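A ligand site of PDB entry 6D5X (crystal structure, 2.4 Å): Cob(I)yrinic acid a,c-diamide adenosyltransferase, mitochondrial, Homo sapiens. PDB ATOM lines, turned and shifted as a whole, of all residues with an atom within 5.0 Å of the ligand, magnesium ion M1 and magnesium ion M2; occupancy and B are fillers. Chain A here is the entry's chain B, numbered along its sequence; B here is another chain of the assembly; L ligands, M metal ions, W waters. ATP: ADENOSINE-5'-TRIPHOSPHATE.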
ATOM      1  N   ILE A   4      38.621 -29.454   7.288  1.00  0.00           N
ATOM      2  CA  ILE A   4      37.286 -29.985   7.055  1.00  0.00           C
ATOM      3  C   ILE A   4      36.289 -28.870   6.755  1.00  0.00           C
ATOM      4  O   ILE A   4      35.372 -29.047   5.949  1.00  0.00           O
ATOM      5  CB  ILE A   4      36.853 -30.842   8.265  1.00  0.00           C
ATOM      6  CG1 ILE A   4      37.689 -32.129   8.348  1.00  0.00           C
ATOM      7  CG2 ILE A   4      35.372 -31.181   8.198  1.00  0.00           C
ATOM      8  CD1 ILE A   4      39.066 -31.963   8.974  1.00  0.00           C
ATOM      9  N   TYR A   5      36.453 -27.720   7.392  1.00  0.00           N
ATOM     10  CA  TYR A   5      35.594 -26.561   7.218  1.00  0.00           C
ATOM     11  C   TYR A   5      36.250 -25.550   6.285  1.00  0.00           C
ATOM     12  O   TYR A   5      37.471 -25.484   6.181  1.00  0.00           O
ATOM     13  CB  TYR A   5      35.294 -25.921   8.569  1.00  0.00           C
ATOM     14  CG  TYR A   5      36.535 -25.737   9.417  1.00  0.00           C
ATOM     15  CD1 TYR A   5      36.988 -26.748  10.254  1.00  0.00           C
ATOM     16  CD2 TYR A   5      37.268 -24.554   9.371  1.00  0.00           C
ATOM     17  CE1 TYR A   5      38.122 -26.600  11.029  1.00  0.00           C
ATOM     18  CE2 TYR A   5      38.420 -24.396  10.135  1.00  0.00           C
ATOM     19  CZ  TYR A   5      38.829 -25.419  10.959  1.00  0.00           C
ATOM     20  OH  TYR A   5      39.968 -25.264  11.729  1.00  0.00           O
ATOM     21  N   THR A   6      35.420 -24.752   5.603  1.00  0.00           N
ATOM     22  CA  THR A   6      35.920 -23.726   4.696  1.00  0.00           C
ATOM     23  C   THR A   6      35.821 -22.316   5.264  1.00  0.00           C
ATOM     24  O   THR A   6      36.582 -21.444   4.826  1.00  0.00           O
ATOM     25  CB  THR A   6      35.160 -23.760   3.352  1.00  0.00           C
ATOM     26  OG1 THR A   6      33.812 -23.319   3.537  1.00  0.00           O
ATOM     27  CG2 THR A   6      35.169 -25.162   2.778  1.00  0.00           C
ATOM     28  N   LYS A   7      34.899 -22.080   6.196  1.00  0.00           N
ATOM     29  CA  LYS A   7      34.574 -20.806   6.829  1.00  0.00           C
ATOM     30  C   LYS A   7      33.730 -19.925   5.901  1.00  0.00           C
ATOM     31  O   LYS A   7      33.350 -18.821   6.313  1.00  0.00           O
ATOM     32  CB  LYS A   7      35.813 -20.007   7.275  1.00  0.00           C
ATOM     33  CG  LYS A   7      36.581 -20.628   8.438  1.00  0.00           C
ATOM     34  CD  LYS A   7      37.698 -19.703   8.897  1.00  0.00           C
ATOM     35  CE  LYS A   7      38.403 -20.258  10.131  1.00  0.00           C
ATOM     36  NZ  LYS A   7      39.500 -19.366  10.603  1.00  0.00           N
ATOM     37  N   THR A   8      33.414 -20.367   4.687  1.00  0.00           N
ATOM     38  CA  THR A   8      32.606 -19.578   3.760  1.00  0.00           C
ATOM     39  C   THR A   8      31.165 -19.391   4.230  1.00  0.00           C
ATOM     40  O   THR A   8      30.453 -18.579   3.640  1.00  0.00           O
ATOM     41  CB  THR A   8      32.611 -20.235   2.375  1.00  0.00           C
ATOM     42  OG1 THR A   8      32.076 -21.556   2.470  1.00  0.00           O
ATOM     43  CG2 THR A   8      34.032 -20.298   1.831  1.00  0.00           C
ATOM     44  N   GLY A   9      30.728 -20.116   5.247  1.00  0.00           N
ATOM     45  CA  GLY A   9      29.408 -19.966   5.799  1.00  0.00           C
ATOM     46  C   GLY A   9      29.365 -19.236   7.123  1.00  0.00           C
ATOM     47  O   GLY A   9      28.329 -19.242   7.786  1.00  0.00           O
ATOM     48  N   ASP A  10      30.462 -18.584   7.523  1.00  0.00           N
ATOM     49  CA  ASP A  10      30.514 -17.888   8.805  1.00  0.00           C
ATOM     50  C   ASP A  10      29.654 -16.628   8.830  1.00  0.00           C
ATOM     51  O   ASP A  10      29.255 -16.189   9.920  1.00  0.00           O
ATOM     52  CB  ASP A  10      31.958 -17.527   9.139  1.00  0.00           C
ATOM     53  CG  ASP A  10      32.751 -18.715   9.655  1.00  0.00           C
ATOM     54  OD1 ASP A  10      32.144 -19.767   9.965  1.00  0.00           O
ATOM     55  OD2 ASP A  10      33.987 -18.599   9.770  1.00  0.00           O
ATOM     56  N   PHE A  13      25.544 -17.355   5.048  1.00  0.00           N
ATOM     57  CA  PHE A  13      25.105 -17.667   3.688  1.00  0.00           C
ATOM     58  C   PHE A  13      25.667 -19.027   3.290  1.00  0.00           C
ATOM     59  O   PHE A  13      26.711 -19.459   3.795  1.00  0.00           O
ATOM     60  CB  PHE A  13      25.567 -16.584   2.680  1.00  0.00           C
ATOM     61  CG  PHE A  13      24.950 -15.230   2.922  1.00  0.00           C
ATOM     62  CD1 PHE A  13      25.637 -14.269   3.633  1.00  0.00           C
ATOM     63  CD2 PHE A  13      23.666 -14.938   2.465  1.00  0.00           C
ATOM     64  CE1 PHE A  13      25.078 -13.030   3.880  1.00  0.00           C
ATOM     65  CE2 PHE A  13      23.098 -13.694   2.713  1.00  0.00           C
ATOM     66  CZ  PHE A  13      23.805 -12.739   3.432  1.00  0.00           C
ATOM     67  N   SER A  14      24.981 -19.695   2.379  1.00  0.00           N
ATOM     68  CA  SER A  14      25.431 -21.004   1.923  1.00  0.00           C
ATOM     69  C   SER A  14      24.994 -21.196   0.484  1.00  0.00           C
ATOM     70  O   SER A  14      24.367 -20.323  -0.125  1.00  0.00           O
ATOM     71  CB  SER A  14      24.912 -22.114   2.835  1.00  0.00           C
ATOM     72  OG  SER A  14      25.738 -23.258   2.735  1.00  0.00           O
ATOM     73  N   SER A  15      25.318 -22.361  -0.065  1.00  0.00           N
ATOM     74  CA  SER A  15      25.117 -22.649  -1.481  1.00  0.00           C
ATOM     75  C   SER A  15      24.072 -23.736  -1.660  1.00  0.00           C
ATOM     76  O   SER A  15      24.046 -24.715  -0.900  1.00  0.00           O
ATOM     77  CB  SER A  15      26.422 -23.118  -2.128  1.00  0.00           C
ATOM     78  OG  SER A  15      27.382 -22.081  -2.167  1.00  0.00           O
ATOM     79  N   THR A  16      23.227 -23.564  -2.664  1.00  0.00           N
ATOM     80  CA  THR A  16      22.405 -24.655  -3.178  1.00  0.00           C
ATOM     81  C   THR A  16      23.212 -25.465  -4.194  1.00  0.00           C
ATOM     82  O   THR A  16      24.331 -25.097  -4.584  1.00  0.00           O
ATOM     83  CB  THR A  16      21.131 -24.112  -3.827  1.00  0.00           C
ATOM     84  OG1 THR A  16      21.464 -23.450  -5.058  1.00  0.00           O
ATOM     85  CG2 THR A  16      20.444 -23.129  -2.894  1.00  0.00           C
ATOM     86  N   PHE A  17      22.634 -26.585  -4.628  1.00  0.00           N
ATOM     87  CA  PHE A  17      23.309 -27.417  -5.630  1.00  0.00           C
ATOM     88  C   PHE A  17      23.282 -26.811  -7.030  1.00  0.00           C
ATOM     89  O   PHE A  17      23.903 -27.375  -7.930  1.00  0.00           O
ATOM     90  CB  PHE A  17      22.717 -28.826  -5.620  1.00  0.00           C
ATOM     91  CG  PHE A  17      23.090 -29.644  -4.402  1.00  0.00           C
ATOM     92  CD1 PHE A  17      23.805 -29.066  -3.369  1.00  0.00           C
ATOM     93  CD2 PHE A  17      22.736 -30.978  -4.309  1.00  0.00           C
ATOM     94  CE1 PHE A  17      24.155 -29.804  -2.247  1.00  0.00           C
ATOM     95  CE2 PHE A  17      23.082 -31.724  -3.182  1.00  0.00           C
ATOM     96  CZ  PHE A  17      23.793 -31.133  -2.153  1.00  0.00           C
ATOM     97  N   LYS A  24      21.061 -18.738   5.284  1.00  0.00           N
ATOM     98  CA  LYS A  24      20.876 -20.071   5.831  1.00  0.00           C
ATOM     99  C   LYS A  24      19.478 -20.311   6.402  1.00  0.00           C
ATOM    100  O   LYS A  24      19.148 -21.468   6.701  1.00  0.00           O
ATOM    101  CB  LYS A  24      21.933 -20.360   6.904  1.00  0.00           C
ATOM    102  CG  LYS A  24      23.337 -20.507   6.330  1.00  0.00           C
ATOM    103  CD  LYS A  24      24.319 -21.025   7.377  1.00  0.00           C
ATOM    104  CE  LYS A  24      25.672 -21.324   6.750  1.00  0.00           C
ATOM    105  NZ  LYS A  24      26.688 -21.732   7.747  1.00  0.00           N
ATOM    106  N   PHE A  29      17.042 -24.740   2.968  1.00  0.00           N
ATOM    107  CA  PHE A  29      17.898 -25.270   4.010  1.00  0.00           C
ATOM    108  C   PHE A  29      17.105 -25.799   5.198  1.00  0.00           C
ATOM    109  O   PHE A  29      17.536 -26.759   5.833  1.00  0.00           O
ATOM    110  CB  PHE A  29      18.917 -24.221   4.461  1.00  0.00           C
ATOM    111  CG  PHE A  29      19.830 -23.767   3.341  1.00  0.00           C
ATOM    112  CD1 PHE A  29      19.892 -22.432   2.972  1.00  0.00           C
ATOM    113  CD2 PHE A  29      20.600 -24.689   2.656  1.00  0.00           C
ATOM    114  CE1 PHE A  29      20.722 -22.023   1.946  1.00  0.00           C
ATOM    115  CE2 PHE A  29      21.429 -24.280   1.630  1.00  0.00           C
ATOM    116  CZ  PHE A  29      21.498 -22.952   1.274  1.00  0.00           C
ATOM    117  N   VAL A  32      16.180 -29.286   3.909  1.00  0.00           N
ATOM    118  CA  VAL A  32      17.332 -30.176   3.880  1.00  0.00           C
ATOM    119  C   VAL A  32      17.751 -30.556   5.295  1.00  0.00           C
ATOM    120  O   VAL A  32      18.028 -31.725   5.599  1.00  0.00           O
ATOM    121  CB  VAL A  32      18.486 -29.527   3.103  1.00  0.00           C
ATOM    122  CG1 VAL A  32      19.777 -30.303   3.308  1.00  0.00           C
ATOM    123  CG2 VAL A  32      18.139 -29.442   1.620  1.00  0.00           C
ATOM    124  N   GLY A  33      17.788 -29.567   6.203  1.00  0.00           N
ATOM    125  CA  GLY A  33      18.199 -29.844   7.563  1.00  0.00           C
ATOM    126  C   GLY A  33      17.230 -30.741   8.311  1.00  0.00           C
ATOM    127  O   GLY A  33      17.650 -31.577   9.111  1.00  0.00           O
ATOM    128  N   ARG B 136      22.672 -27.525  13.626  1.00  0.00           N
ATOM    129  CA  ARG B 136      22.459 -26.808  12.367  1.00  0.00           C
ATOM    130  C   ARG B 136      21.109 -26.116  12.352  1.00  0.00           C
ATOM    131  O   ARG B 136      20.986 -24.992  11.822  1.00  0.00           O
ATOM    132  CB  ARG B 136      22.616 -27.777  11.206  1.00  0.00           C
ATOM    133  CG  ARG B 136      24.071 -28.102  10.928  1.00  0.00           C
ATOM    134  CD  ARG B 136      24.277 -29.429  10.225  1.00  0.00           C
ATOM    135  NE  ARG B 136      24.147 -29.320   8.778  1.00  0.00           N
ATOM    136  CZ  ARG B 136      25.030 -28.724   7.977  1.00  0.00           C
ATOM    137  NH1 ARG B 136      26.136 -28.176   8.468  1.00  0.00           N
ATOM    138  NH2 ARG B 136      24.813 -28.687   6.676  1.00  0.00           N
ATOM    139  N   GLU B 139      21.674 -22.985  14.218  1.00  0.00           N
ATOM    140  CA  GLU B 139      22.336 -22.005  13.359  1.00  0.00           C
ATOM    141  C   GLU B 139      21.327 -21.292  12.467  1.00  0.00           C
ATOM    142  O   GLU B 139      21.378 -20.060  12.317  1.00  0.00           O
ATOM    143  CB  GLU B 139      23.425 -22.676  12.522  1.00  0.00           C
ATOM    144  CG  GLU B 139      24.144 -21.715  11.592  1.00  0.00           C
ATOM    145  CD  GLU B 139      25.202 -22.377  10.760  1.00  0.00           C
ATOM    146  OE1 GLU B 139      25.171 -23.621  10.608  1.00  0.00           O
ATOM    147  OE2 GLU B 139      26.087 -21.662  10.254  1.00  0.00           O
ATOM    148  N   ARG B 140      20.417 -22.050  11.861  1.00  0.00           N
ATOM    149  CA  ARG B 140      19.405 -21.401  11.029  1.00  0.00           C
ATOM    150  C   ARG B 140      18.513 -20.473  11.842  1.00  0.00           C
ATOM    151  O   ARG B 140      18.000 -19.497  11.290  1.00  0.00           O
ATOM    152  CB  ARG B 140      18.551 -22.440  10.305  1.00  0.00           C
ATOM    153  CG  ARG B 140      19.326 -23.442   9.505  1.00  0.00           C
ATOM    154  CD  ARG B 140      18.409 -24.155   8.539  1.00  0.00           C
ATOM    155  NE  ARG B 140      17.371 -24.916   9.226  1.00  0.00           N
ATOM    156  CZ  ARG B 140      17.545 -26.144   9.698  1.00  0.00           C
ATOM    157  NH1 ARG B 140      18.696 -26.769   9.558  1.00  0.00           N
ATOM    158  NH2 ARG B 140      16.545 -26.766  10.305  1.00  0.00           N
ATOM    159  N   ASN B 160      28.331 -22.592  13.486  1.00  0.00           N
ATOM    160  CA  ASN B 160      28.785 -23.181  12.229  1.00  0.00           C
ATOM    161  C   ASN B 160      29.977 -24.097  12.466  1.00  0.00           C
ATOM    162  O   ASN B 160      30.056 -25.180  11.868  1.00  0.00           O
ATOM    163  CB  ASN B 160      29.129 -22.062  11.247  1.00  0.00           C
ATOM    164  CG  ASN B 160      29.524 -22.588   9.881  1.00  0.00           C
ATOM    165  OD1 ASN B 160      29.094 -23.664   9.473  1.00  0.00           O
ATOM    166  ND2 ASN B 160      30.343 -21.817   9.163  1.00  0.00           N
ATOM    167  N   ASP B 164      30.859 -28.900  12.704  1.00  0.00           N
ATOM    168  CA  ASP B 164      31.980 -29.708  12.255  1.00  0.00           C
ATOM    169  C   ASP B 164      32.660 -30.411  13.425  1.00  0.00           C
ATOM    170  O   ASP B 164      33.115 -31.558  13.286  1.00  0.00           O
ATOM    171  CB  ASP B 164      32.987 -28.842  11.498  1.00  0.00           C
ATOM    172  CG  ASP B 164      32.445 -28.361  10.170  1.00  0.00           C
ATOM    173  OD1 ASP B 164      32.166 -29.193   9.292  1.00  0.00           O
ATOM    174  OD2 ASP B 164      32.283 -27.129  10.016  1.00  0.00           O
HETATM  175  PG  ATP L   1      31.333 -23.961   6.094  1.00  0.00           P
HETATM  176  O1G ATP L   1      31.561 -22.512   6.480  1.00  0.00           O
HETATM  177  O2G ATP L   1      32.540 -24.663   5.506  1.00  0.00           O
HETATM  178  O3G ATP L   1      30.586 -24.766   7.129  1.00  0.00           O
HETATM  179  PB  ATP L   1      28.728 -24.027   5.026  1.00  0.00           P
HETATM  180  O1B ATP L   1      28.066 -23.062   4.077  1.00  0.00           O
HETATM  181  O2B ATP L   1      28.368 -24.014   6.483  1.00  0.00           O
HETATM  182  O3B ATP L   1      30.318 -23.879   4.844  1.00  0.00           O
HETATM  183  PA  ATP L   1      28.473 -26.828   5.319  1.00  0.00           P
HETATM  184  O1A ATP L   1      29.625 -27.701   4.883  1.00  0.00           O
HETATM  185  O2A ATP L   1      28.364 -26.416   6.760  1.00  0.00           O
HETATM  186  O3A ATP L   1      28.523 -25.505   4.406  1.00  0.00           O
HETATM  187  O5' ATP L   1      27.111 -27.540   4.835  1.00  0.00           O
HETATM  188  C5' ATP L   1      27.093 -28.280   3.613  1.00  0.00           C
HETATM  189  C4' ATP L   1      25.824 -27.967   2.837  1.00  0.00           C
HETATM  190  O4' ATP L   1      24.676 -28.120   3.674  1.00  0.00           O
HETATM  191  C3' ATP L   1      25.798 -26.521   2.344  1.00  0.00           C
HETATM  192  O3' ATP L   1      26.243 -26.442   0.997  1.00  0.00           O
HETATM  193  C2' ATP L   1      24.346 -26.110   2.464  1.00  0.00           C
HETATM  194  O2' ATP L   1      23.677 -26.397   1.227  1.00  0.00           O
HETATM  195  C1' ATP L   1      23.782 -27.000   3.549  1.00  0.00           C
HETATM  196  N9  ATP L   1      23.766 -26.301   4.854  1.00  0.00           N
HETATM  197  C8  ATP L   1      24.756 -25.525   5.348  1.00  0.00           C
HETATM  198  N7  ATP L   1      24.436 -25.041   6.576  1.00  0.00           N
HETATM  199  C5  ATP L   1      23.222 -25.519   6.895  1.00  0.00           C
HETATM  200  C6  ATP L   1      22.297 -25.392   8.046  1.00  0.00           C
HETATM  201  N6  ATP L   1      22.620 -24.651   9.127  1.00  0.00           N
HETATM  202  N1  ATP L   1      21.121 -26.054   7.982  1.00  0.00           N
HETATM  203  C2  ATP L   1      20.785 -26.796   6.907  1.00  0.00           C
HETATM  204  N3  ATP L   1      21.577 -26.951   5.834  1.00  0.00           N
HETATM  205  C4  ATP L   1      22.784 -26.345   5.760  1.00  0.00           C
HETATM  206 MG    MG M   1      31.439 -28.704   5.220  1.00  0.00          MG
HETATM  207 MG    MG M   2      28.722 -25.126   8.101  1.00  0.00          MG
HETATM  208  O   HOH W   1      32.649 -30.144   6.042  1.00  0.00           O
HETATM  209  O   HOH W   2      30.178 -29.824   6.408  1.00  0.00           O
HETATM  210  O   HOH W   3      26.610 -24.785   8.608  1.00  0.00           O
HETATM  211  O   HOH W   4      31.665 -27.375   6.866  1.00  0.00           O
HETATM  212  O   HOH W   5      23.388 -30.860   2.928  1.00  0.00           O
HETATM  213  O   HOH W   6      32.442 -27.168   4.416  1.00  0.00           O
HETATM  214  O   HOH W   7      32.374 -24.569   9.703  1.00  0.00           O
HETATM  215  O   HOH W   8      22.508 -30.022   5.982  1.00  0.00           O
HETATM  216  O   HOH W   9      30.922 -29.907   3.456  1.00  0.00           O
HETATM  217  O   HOH W  10      29.464 -21.351   2.134  1.00  0.00           O
HETATM  218  O   HOH W  11      29.431 -26.350   9.742  1.00  0.00           O
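NH1 of Arg 140 of chain B is in hydrogen-bond range of N1 of the ligand (3.0 Å).
O1G of the ligand is in hydrogen-bond range of N of Lys 7.
N of Thr 8 sits at hydrogen-bond distance from O1G of the ligand, 3.4 Å away.
N6 of the ligand sits at hydrogen-bond distance from O of Arg 136 of chain B.
An oxygen (O2B) of the ligand sits close to the side-chain amino group (NZ) of Lys 24, at 3.1 Å.
An oxygen (O4') of the ligand lies within hydrogen-bond range of the guanidinium group of Arg 136 of chain B, at 3.1 Å.
A nitrogen (N6) of the ligand lies within hydrogen-bond range of the side-chain carboxylate (OE1) of Glu 139 of chain B.
The backbone NH (N) of Gly 9 lies within hydrogen-bond range of an oxygen (O1G) of the ligand (2.8 Å).
The backbone carbonyl oxygen (O) of Ser 15 sits at hydrogen-bond distance from an oxygen (O2') of the ligand (2.7 Å).
The side-chain hydroxyl (OG) of Ser 14 is in hydrogen-bond range of an oxygen (O1B) of the ligand (2.7 Å).
The backbone NH (N) of Thr 6 lies within hydrogen-bond range of an oxygen (O2G) of the ligand, 2.9 Å away.
O2G of the ligand sits at hydrogen-bond distance from OG1 of Thr 6 (2.7 Å).
NZ of Lys 24 lies within hydrogen-bond range of O of Gly 9, 3.0 Å away.
OG1 of Thr 8 lies within hydrogen-bond range of OG1 of Thr 6, 2.7 Å away.
The side-chain amino group (NZ) of Lys 24 is in salt-bridge range of the side-chain carboxylate (OE2) of Glu 139 of chain B.
ND2 of Asn 160 of chain B is in hydrogen-bond range of OD1 of Asp 10, 2.8 Å away.
Tyr 5 touches the ligand (C to O2G, 3.9 Å).
Phe 13 touches the ligand.
Phe 29 touches the ligand (CE2 to O2', 3.1 Å).
14 residues have an atom within 4 Å of the ligand: Tyr 5, Thr 6, Lys 7, Thr 8, Gly 9, Phe 13, Ser 14, Ser 15, Lys 24, Phe 29, Arg 136 of chain B, Glu 139 of chain B, Arg 140 of chain B and Asn 160 of chain B.
The nearest printed residue that does not touch the ligand is Gly 33 (4.1 Å).
No residue comes within 4 Å of magnesium ion M1.
The nearest printed residue that does not touch magnesium ion M1 is Ile 4 (4.01 Å).
NZ of Lys 24 touches magnesium ion M2, 3.97 Å away.
The nearest printed residue that does not touch magnesium ion M2 is Arg 136 of chain B (4.02 Å).
Magnesium ion M1 is bound by water W6 (2.0 Å), water W1 (2.1 Å), water W2 (2.1 Å), an oxygen (O1A) of the ligand (2.1 Å), water W4 (2.1 Å) and water W9 (2.2 Å).
Magnesium ion M1 has six donor atoms within binding distance.
Magnesium ion M2 is bound by an oxygen (O2A) of the ligand (1.9 Å), an oxygen (O2B) of the ligand (2.0 Å), the side-chain amide oxygen of Asn 160 of chain B (2.0 Å), an oxygen (O3G) of the ligand (2.1 Å), water W11 (2.2 Å) and water W3 (2.2 Å).
Water W4 bridges OD1 of Asp 164 of chain B and O2G of the ligand.
Water W11 lies within hydrogen-bond range of the backbone carbonyl oxygen of Asn 160 of chain B (2.5 Å) and the side-chain carboxylate of Asp 164 of chain B (3.0 Å).
Water W3 lies within hydrogen-bond range of the side-chain carboxylate of Glu 139 of chain B (2.7 Å), a nitrogen (N7) of the ligand (3.0 Å), the side-chain amino group of Lys 24 (3.2 Å) and the guanidinium group of Arg 136 of chain B (3.4 Å).
Water W10 bridges the side-chain hydroxyl (OG1) of Thr 8 and an oxygen (O1B) of the ligand.
Water W7 lies within hydrogen-bond range of OD2 of Asp 164 of chain B (2.6 Å) and O of Asn 160 of chain B (3.2 Å).
Water W8 bridges NH2 of Arg 136 of chain B and N3 of the ligand.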
